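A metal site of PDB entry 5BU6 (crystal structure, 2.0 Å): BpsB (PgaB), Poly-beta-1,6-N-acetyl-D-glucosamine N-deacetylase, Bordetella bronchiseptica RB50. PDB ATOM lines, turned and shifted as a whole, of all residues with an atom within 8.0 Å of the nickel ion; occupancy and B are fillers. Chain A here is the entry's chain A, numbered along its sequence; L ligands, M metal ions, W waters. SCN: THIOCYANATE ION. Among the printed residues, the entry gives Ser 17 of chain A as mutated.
OH of Tyr 222 is in hydrogen-bond range of O of His 159 (3.2 Å).
O of Val 219 is in hydrogen-bond range of ND1 of His 154.
N of Asp 84 lies within hydrogen-bond range of O of Ala 107, at 2.9 Å.
Within 4 Å of the nickel ion: Asp 84, His 154 and His 159.
The nearest printed residue that does not touch the nickel ion is Asp 83 (4.2 Å).
NE2 of His 159 is bound to the nickel ion, 2.1 Å away.
OD1 of Asp 84 binds the nickel ion (2.1 Å).
Water W1 binds the nickel ion (2.1 Å).
S of the ligand is bound to the nickel ion (2.1 Å).
Water W2 binds the nickel ion (2.2 Å).
The nickel ion is bound by NE2 of His 154.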
ATOM      1  N   SER A  17      16.173  35.367 -15.307  1.00  0.00           N
ATOM      2  CA  SER A  17      15.064  34.422 -15.237  1.00  0.00           C
ATOM      3  C   SER A  17      13.972  35.007 -14.333  1.00  0.00           C
ATOM      4  O   SER A  17      14.239  35.380 -13.200  1.00  0.00           O
ATOM      5  CB  SER A  17      15.581  33.075 -14.729  1.00  0.00           C
ATOM      6  OG  SER A  17      14.551  32.114 -14.599  1.00  0.00           O
ATOM      7  N   HIS A  19      10.317  35.075 -12.326  1.00  0.00           N
ATOM      8  CA  HIS A  19       9.410  34.159 -11.631  1.00  0.00           C
ATOM      9  C   HIS A  19       8.270  34.980 -11.034  1.00  0.00           C
ATOM     10  O   HIS A  19       8.511  35.971 -10.327  1.00  0.00           O
ATOM     11  CB  HIS A  19      10.191  33.393 -10.555  1.00  0.00           C
ATOM     12  CG  HIS A  19       9.376  32.405  -9.773  1.00  0.00           C
ATOM     13  ND1 HIS A  19       9.010  31.175 -10.267  1.00  0.00           N
ATOM     14  CD2 HIS A  19       8.881  32.464  -8.514  1.00  0.00           C
ATOM     15  CE1 HIS A  19       8.318  30.524  -9.361  1.00  0.00           C
ATOM     16  NE2 HIS A  19       8.219  31.285  -8.285  1.00  0.00           N
ATOM     17  N   LEU A  25       5.514  28.096  -5.580  1.00  0.00           N
ATOM     18  CA  LEU A  25       6.127  26.813  -5.311  1.00  0.00           C
ATOM     19  C   LEU A  25       7.642  26.897  -5.514  1.00  0.00           C
ATOM     20  O   LEU A  25       8.146  26.774  -6.628  1.00  0.00           O
ATOM     21  CB  LEU A  25       5.536  25.708  -6.192  1.00  0.00           C
ATOM     22  CG  LEU A  25       5.887  24.336  -5.633  1.00  0.00           C
ATOM     23  CD1 LEU A  25       5.141  24.066  -4.330  1.00  0.00           C
ATOM     24  CD2 LEU A  25       5.640  23.234  -6.645  1.00  0.00           C
ATOM     25  N   MET A  32      18.199  26.837  -4.181  1.00  0.00           N
ATOM     26  CA  MET A  32      18.015  28.025  -5.007  1.00  0.00           C
ATOM     27  C   MET A  32      18.991  29.125  -4.600  1.00  0.00           C
ATOM     28  O   MET A  32      19.529  29.098  -3.498  1.00  0.00           O
ATOM     29  CB  MET A  32      16.570  28.520  -4.908  1.00  0.00           C
ATOM     30  CG  MET A  32      15.528  27.455  -5.212  1.00  0.00           C
ATOM     31  SD  MET A  32      15.867  26.544  -6.746  1.00  0.00           S
ATOM     32  CE  MET A  32      14.453  27.030  -7.740  1.00  0.00           C
ATOM     33  N   PHE A  82      11.301  33.039 -19.111  1.00  0.00           N
ATOM     34  CA  PHE A  82      10.076  32.820 -18.350  1.00  0.00           C
ATOM     35  C   PHE A  82       9.750  31.319 -18.352  1.00  0.00           C
ATOM     36  O   PHE A  82       9.320  30.793 -19.375  1.00  0.00           O
ATOM     37  CB  PHE A  82       8.917  33.626 -18.946  1.00  0.00           C
ATOM     38  CG  PHE A  82       9.139  35.100 -18.957  1.00  0.00           C
ATOM     39  CD1 PHE A  82       9.816  35.710 -20.014  1.00  0.00           C
ATOM     40  CD2 PHE A  82       8.707  35.887 -17.906  1.00  0.00           C
ATOM     41  CE1 PHE A  82      10.055  37.071 -20.024  1.00  0.00           C
ATOM     42  CE2 PHE A  82       8.932  37.263 -17.901  1.00  0.00           C
ATOM     43  CZ  PHE A  82       9.615  37.858 -18.965  1.00  0.00           C
ATOM     44  N   ASP A  83       9.979  30.632 -17.243  1.00  0.00           N
ATOM     45  CA  ASP A  83       9.770  29.171 -17.246  1.00  0.00           C
ATOM     46  C   ASP A  83       8.474  28.771 -16.536  1.00  0.00           C
ATOM     47  O   ASP A  83       7.898  29.561 -15.809  1.00  0.00           O
ATOM     48  CB  ASP A  83      10.942  28.436 -16.599  1.00  0.00           C
ATOM     49  CG  ASP A  83      12.197  29.294 -16.477  1.00  0.00           C
ATOM     50  OD1 ASP A  83      12.652  29.857 -17.493  1.00  0.00           O
ATOM     51  OD2 ASP A  83      12.727  29.408 -15.342  1.00  0.00           O
ATOM     52  N   ASP A  84       8.047  27.526 -16.799  1.00  0.00           N
ATOM     53  CA  ASP A  84       6.994  26.776 -16.078  1.00  0.00           C
ATOM     54  C   ASP A  84       5.682  26.785 -16.848  1.00  0.00           C
ATOM     55  O   ASP A  84       4.842  25.927 -16.638  1.00  0.00           O
ATOM     56  CB  ASP A  84       6.756  27.268 -14.650  1.00  0.00           C
ATOM     57  CG  ASP A  84       7.880  26.900 -13.696  1.00  0.00           C
ATOM     58  OD1 ASP A  84       8.922  26.391 -14.141  1.00  0.00           O
ATOM     59  OD2 ASP A  84       7.712  27.124 -12.474  1.00  0.00           O
ATOM     60  N   GLY A  85       5.509  27.753 -17.743  1.00  0.00           N
ATOM     61  CA  GLY A  85       4.398  27.717 -18.668  1.00  0.00           C
ATOM     62  C   GLY A  85       3.027  27.990 -18.061  1.00  0.00           C
ATOM     63  O   GLY A  85       2.007  27.534 -18.583  1.00  0.00           O
ATOM     64  N   TYR A  86       2.996  28.742 -16.964  1.00  0.00           N
ATOM     65  CA  TYR A  86       1.709  29.155 -16.404  1.00  0.00           C
ATOM     66  C   TYR A  86       0.942  30.090 -17.346  1.00  0.00           C
ATOM     67  O   TYR A  86       1.532  30.694 -18.237  1.00  0.00           O
ATOM     68  CB  TYR A  86       1.919  29.811 -15.039  1.00  0.00           C
ATOM     69  CG  TYR A  86       2.172  28.812 -13.920  1.00  0.00           C
ATOM     70  CD1 TYR A  86       1.097  28.168 -13.288  1.00  0.00           C
ATOM     71  CD2 TYR A  86       3.454  28.515 -13.487  1.00  0.00           C
ATOM     72  CE1 TYR A  86       1.316  27.269 -12.255  1.00  0.00           C
ATOM     73  CE2 TYR A  86       3.675  27.609 -12.467  1.00  0.00           C
ATOM     74  CZ  TYR A  86       2.610  27.001 -11.854  1.00  0.00           C
ATOM     75  OH  TYR A  86       2.836  26.102 -10.829  1.00  0.00           O
ATOM     76  N   ALA A 107      10.202  28.411 -21.263  1.00  0.00           N
ATOM     77  CA  ALA A 107      10.598  27.018 -21.073  1.00  0.00           C
ATOM     78  C   ALA A 107       9.401  26.249 -20.499  1.00  0.00           C
ATOM     79  O   ALA A 107       8.815  26.657 -19.478  1.00  0.00           O
ATOM     80  CB  ALA A 107      11.811  26.918 -20.147  1.00  0.00           C
ATOM     81  N   VAL A 109       7.365  22.865 -19.110  1.00  0.00           N
ATOM     82  CA  VAL A 109       7.419  21.539 -18.500  1.00  0.00           C
ATOM     83  C   VAL A 109       6.346  20.710 -19.191  1.00  0.00           C
ATOM     84  O   VAL A 109       5.156  20.925 -18.988  1.00  0.00           O
ATOM     85  CB  VAL A 109       7.151  21.551 -16.987  1.00  0.00           C
ATOM     86  CG1 VAL A 109       7.292  20.139 -16.431  1.00  0.00           C
ATOM     87  CG2 VAL A 109       8.100  22.523 -16.263  1.00  0.00           C
ATOM     88  N   TRP A 112       3.253  18.947 -17.722  1.00  0.00           N
ATOM     89  CA  TRP A 112       2.258  19.865 -17.195  1.00  0.00           C
ATOM     90  C   TRP A 112       1.373  20.414 -18.298  1.00  0.00           C
ATOM     91  O   TRP A 112       0.164  20.319 -18.248  1.00  0.00           O
ATOM     92  CB  TRP A 112       2.951  21.032 -16.452  1.00  0.00           C
ATOM     93  CG  TRP A 112       3.707  20.648 -15.238  1.00  0.00           C
ATOM     94  CD1 TRP A 112       3.786  19.421 -14.674  1.00  0.00           C
ATOM     95  CD2 TRP A 112       4.524  21.509 -14.417  1.00  0.00           C
ATOM     96  NE1 TRP A 112       4.586  19.446 -13.561  1.00  0.00           N
ATOM     97  CE2 TRP A 112       5.035  20.726 -13.374  1.00  0.00           C
ATOM     98  CE3 TRP A 112       4.851  22.855 -14.481  1.00  0.00           C
ATOM     99  CZ2 TRP A 112       5.878  21.239 -12.389  1.00  0.00           C
ATOM    100  CZ3 TRP A 112       5.686  23.390 -13.477  1.00  0.00           C
ATOM    101  CH2 TRP A 112       6.187  22.571 -12.456  1.00  0.00           C
ATOM    102  N   HIS A 154      11.700  22.727 -20.332  1.00  0.00           N
ATOM    103  CA  HIS A 154      11.919  22.788 -18.885  1.00  0.00           C
ATOM    104  C   HIS A 154      11.814  21.380 -18.314  1.00  0.00           C
ATOM    105  O   HIS A 154      11.417  21.197 -17.165  1.00  0.00           O
ATOM    106  CB  HIS A 154      10.912  23.734 -18.220  1.00  0.00           C
ATOM    107  CG  HIS A 154      11.408  24.350 -16.945  1.00  0.00           C
ATOM    108  ND1 HIS A 154      12.734  24.357 -16.584  1.00  0.00           N
ATOM    109  CD2 HIS A 154      10.741  24.978 -15.946  1.00  0.00           C
ATOM    110  CE1 HIS A 154      12.863  24.944 -15.404  1.00  0.00           C
ATOM    111  NE2 HIS A 154      11.675  25.356 -15.011  1.00  0.00           N
ATOM    112  N   HIS A 159      10.688  18.320 -13.142  1.00  0.00           N
ATOM    113  CA  HIS A 159      10.471  19.522 -12.345  1.00  0.00           C
ATOM    114  C   HIS A 159       9.835  19.144 -11.006  1.00  0.00           C
ATOM    115  O   HIS A 159       8.757  19.625 -10.648  1.00  0.00           O
ATOM    116  CB  HIS A 159       9.601  20.521 -13.123  1.00  0.00           C
ATOM    117  CG  HIS A 159       9.809  21.952 -12.725  1.00  0.00           C
ATOM    118  ND1 HIS A 159       9.669  22.387 -11.425  1.00  0.00           N
ATOM    119  CD2 HIS A 159      10.111  23.047 -13.452  1.00  0.00           C
ATOM    120  CE1 HIS A 159       9.904  23.691 -11.370  1.00  0.00           C
ATOM    121  NE2 HIS A 159      10.174  24.117 -12.585  1.00  0.00           N
ATOM    122  N   VAL A 219      16.271  24.325 -20.040  1.00  0.00           N
ATOM    123  CA  VAL A 219      16.407  25.082 -18.801  1.00  0.00           C
ATOM    124  C   VAL A 219      16.228  24.090 -17.674  1.00  0.00           C
ATOM    125  O   VAL A 219      15.129  23.589 -17.490  1.00  0.00           O
ATOM    126  CB  VAL A 219      15.356  26.207 -18.656  1.00  0.00           C
ATOM    127  CG1 VAL A 219      15.570  26.955 -17.303  1.00  0.00           C
ATOM    128  CG2 VAL A 219      15.438  27.180 -19.833  1.00  0.00           C
ATOM    129  N   TRP A 220      17.296  23.794 -16.949  1.00  0.00           N
ATOM    130  CA  TRP A 220      17.261  22.751 -15.947  1.00  0.00           C
ATOM    131  C   TRP A 220      16.417  23.197 -14.742  1.00  0.00           C
ATOM    132  O   TRP A 220      16.719  24.201 -14.142  1.00  0.00           O
ATOM    133  CB  TRP A 220      18.692  22.416 -15.499  1.00  0.00           C
ATOM    134  CG  TRP A 220      19.556  21.807 -16.615  1.00  0.00           C
ATOM    135  CD1 TRP A 220      20.597  22.402 -17.305  1.00  0.00           C
ATOM    136  CD2 TRP A 220      19.459  20.474 -17.130  1.00  0.00           C
ATOM    137  NE1 TRP A 220      21.127  21.521 -18.224  1.00  0.00           N
ATOM    138  CE2 TRP A 220      20.449  20.336 -18.133  1.00  0.00           C
ATOM    139  CE3 TRP A 220      18.611  19.382 -16.843  1.00  0.00           C
ATOM    140  CZ2 TRP A 220      20.626  19.148 -18.845  1.00  0.00           C
ATOM    141  CZ3 TRP A 220      18.788  18.209 -17.555  1.00  0.00           C
ATOM    142  CH2 TRP A 220      19.778  18.099 -18.559  1.00  0.00           C
ATOM    143  N   PRO A 221      15.379  22.419 -14.390  1.00  0.00           N
ATOM    144  CA  PRO A 221      14.655  22.729 -13.140  1.00  0.00           C
ATOM    145  C   PRO A 221      15.592  22.816 -11.954  1.00  0.00           C
ATOM    146  O   PRO A 221      16.494  21.974 -11.830  1.00  0.00           O
ATOM    147  CB  PRO A 221      13.690  21.548 -12.988  1.00  0.00           C
ATOM    148  CG  PRO A 221      13.400  21.148 -14.429  1.00  0.00           C
ATOM    149  CD  PRO A 221      14.740  21.329 -15.137  1.00  0.00           C
ATOM    150  N   TYR A 222      15.377  23.827 -11.111  1.00  0.00           N
ATOM    151  CA  TYR A 222      16.142  24.022  -9.895  1.00  0.00           C
ATOM    152  C   TYR A 222      17.640  24.191 -10.183  1.00  0.00           C
ATOM    153  O   TYR A 222      18.435  24.098  -9.264  1.00  0.00           O
ATOM    154  CB  TYR A 222      15.918  22.861  -8.931  1.00  0.00           C
ATOM    155  CG  TYR A 222      14.470  22.437  -8.827  1.00  0.00           C
ATOM    156  CD1 TYR A 222      13.527  23.262  -8.224  1.00  0.00           C
ATOM    157  CD2 TYR A 222      14.045  21.208  -9.320  1.00  0.00           C
ATOM    158  CE1 TYR A 222      12.203  22.879  -8.128  1.00  0.00           C
ATOM    159  CE2 TYR A 222      12.721  20.811  -9.224  1.00  0.00           C
ATOM    160  CZ  TYR A 222      11.809  21.649  -8.633  1.00  0.00           C
ATOM    161  OH  TYR A 222      10.490  21.273  -8.532  1.00  0.00           O
ATOM    162  N   GLY A 223      17.995  24.453 -11.440  1.00  0.00           N
ATOM    163  CA  GLY A 223      19.395  24.526 -11.831  1.00  0.00           C
ATOM    164  C   GLY A 223      20.160  23.219 -11.653  1.00  0.00           C
ATOM    165  O   GLY A 223      21.392  23.214 -11.585  1.00  0.00           O
ATOM    166  N   ARG A 260      22.570  32.419 -15.129  1.00  0.00           N
ATOM    167  CA  ARG A 260      21.496  33.390 -15.045  1.00  0.00           C
ATOM    168  C   ARG A 260      21.188  33.813 -13.628  1.00  0.00           C
ATOM    169  O   ARG A 260      21.549  33.117 -12.670  1.00  0.00           O
ATOM    170  CB  ARG A 260      20.230  32.839 -15.700  1.00  0.00           C
ATOM    171  CG  ARG A 260      19.571  31.750 -14.963  1.00  0.00           C
ATOM    172  CD  ARG A 260      18.864  30.789 -15.967  1.00  0.00           C
ATOM    173  NE  ARG A 260      18.279  29.691 -15.217  1.00  0.00           N
ATOM    174  CZ  ARG A 260      16.983  29.442 -15.137  1.00  0.00           C
ATOM    175  NH1 ARG A 260      16.108  30.179 -15.822  1.00  0.00           N
ATOM    176  NH2 ARG A 260      16.553  28.427 -14.407  1.00  0.00           N
ATOM    177  N   LEU A 262      18.115  35.156 -10.954  1.00  0.00           N
ATOM    178  CA  LEU A 262      16.704  34.873 -10.763  1.00  0.00           C
ATOM    179  C   LEU A 262      16.070  36.103 -10.150  1.00  0.00           C
ATOM    180  O   LEU A 262      16.602  36.657  -9.195  1.00  0.00           O
ATOM    181  CB  LEU A 262      16.540  33.641  -9.865  1.00  0.00           C
ATOM    182  CG  LEU A 262      15.152  33.074  -9.621  1.00  0.00           C
ATOM    183  CD1 LEU A 262      14.495  32.686 -10.926  1.00  0.00           C
ATOM    184  CD2 LEU A 262      15.246  31.880  -8.689  1.00  0.00           C
HETATM  185  S   SCN L   1      12.661  25.923 -12.240  1.00  0.00           S
HETATM  186  C   SCN L   1      14.218  26.797 -11.892  1.00  0.00           C
HETATM  187  N   SCN L   1      15.181  27.333 -11.670  1.00  0.00           N
HETATM  188 NI    NI M   1      10.734  26.034 -13.147  1.00  0.00          NI
HETATM  189  O   HOH W   1      11.159  28.074 -13.592  1.00  0.00           O
HETATM  190  O   HOH W   2       9.912  26.930 -11.353  1.00  0.00           O
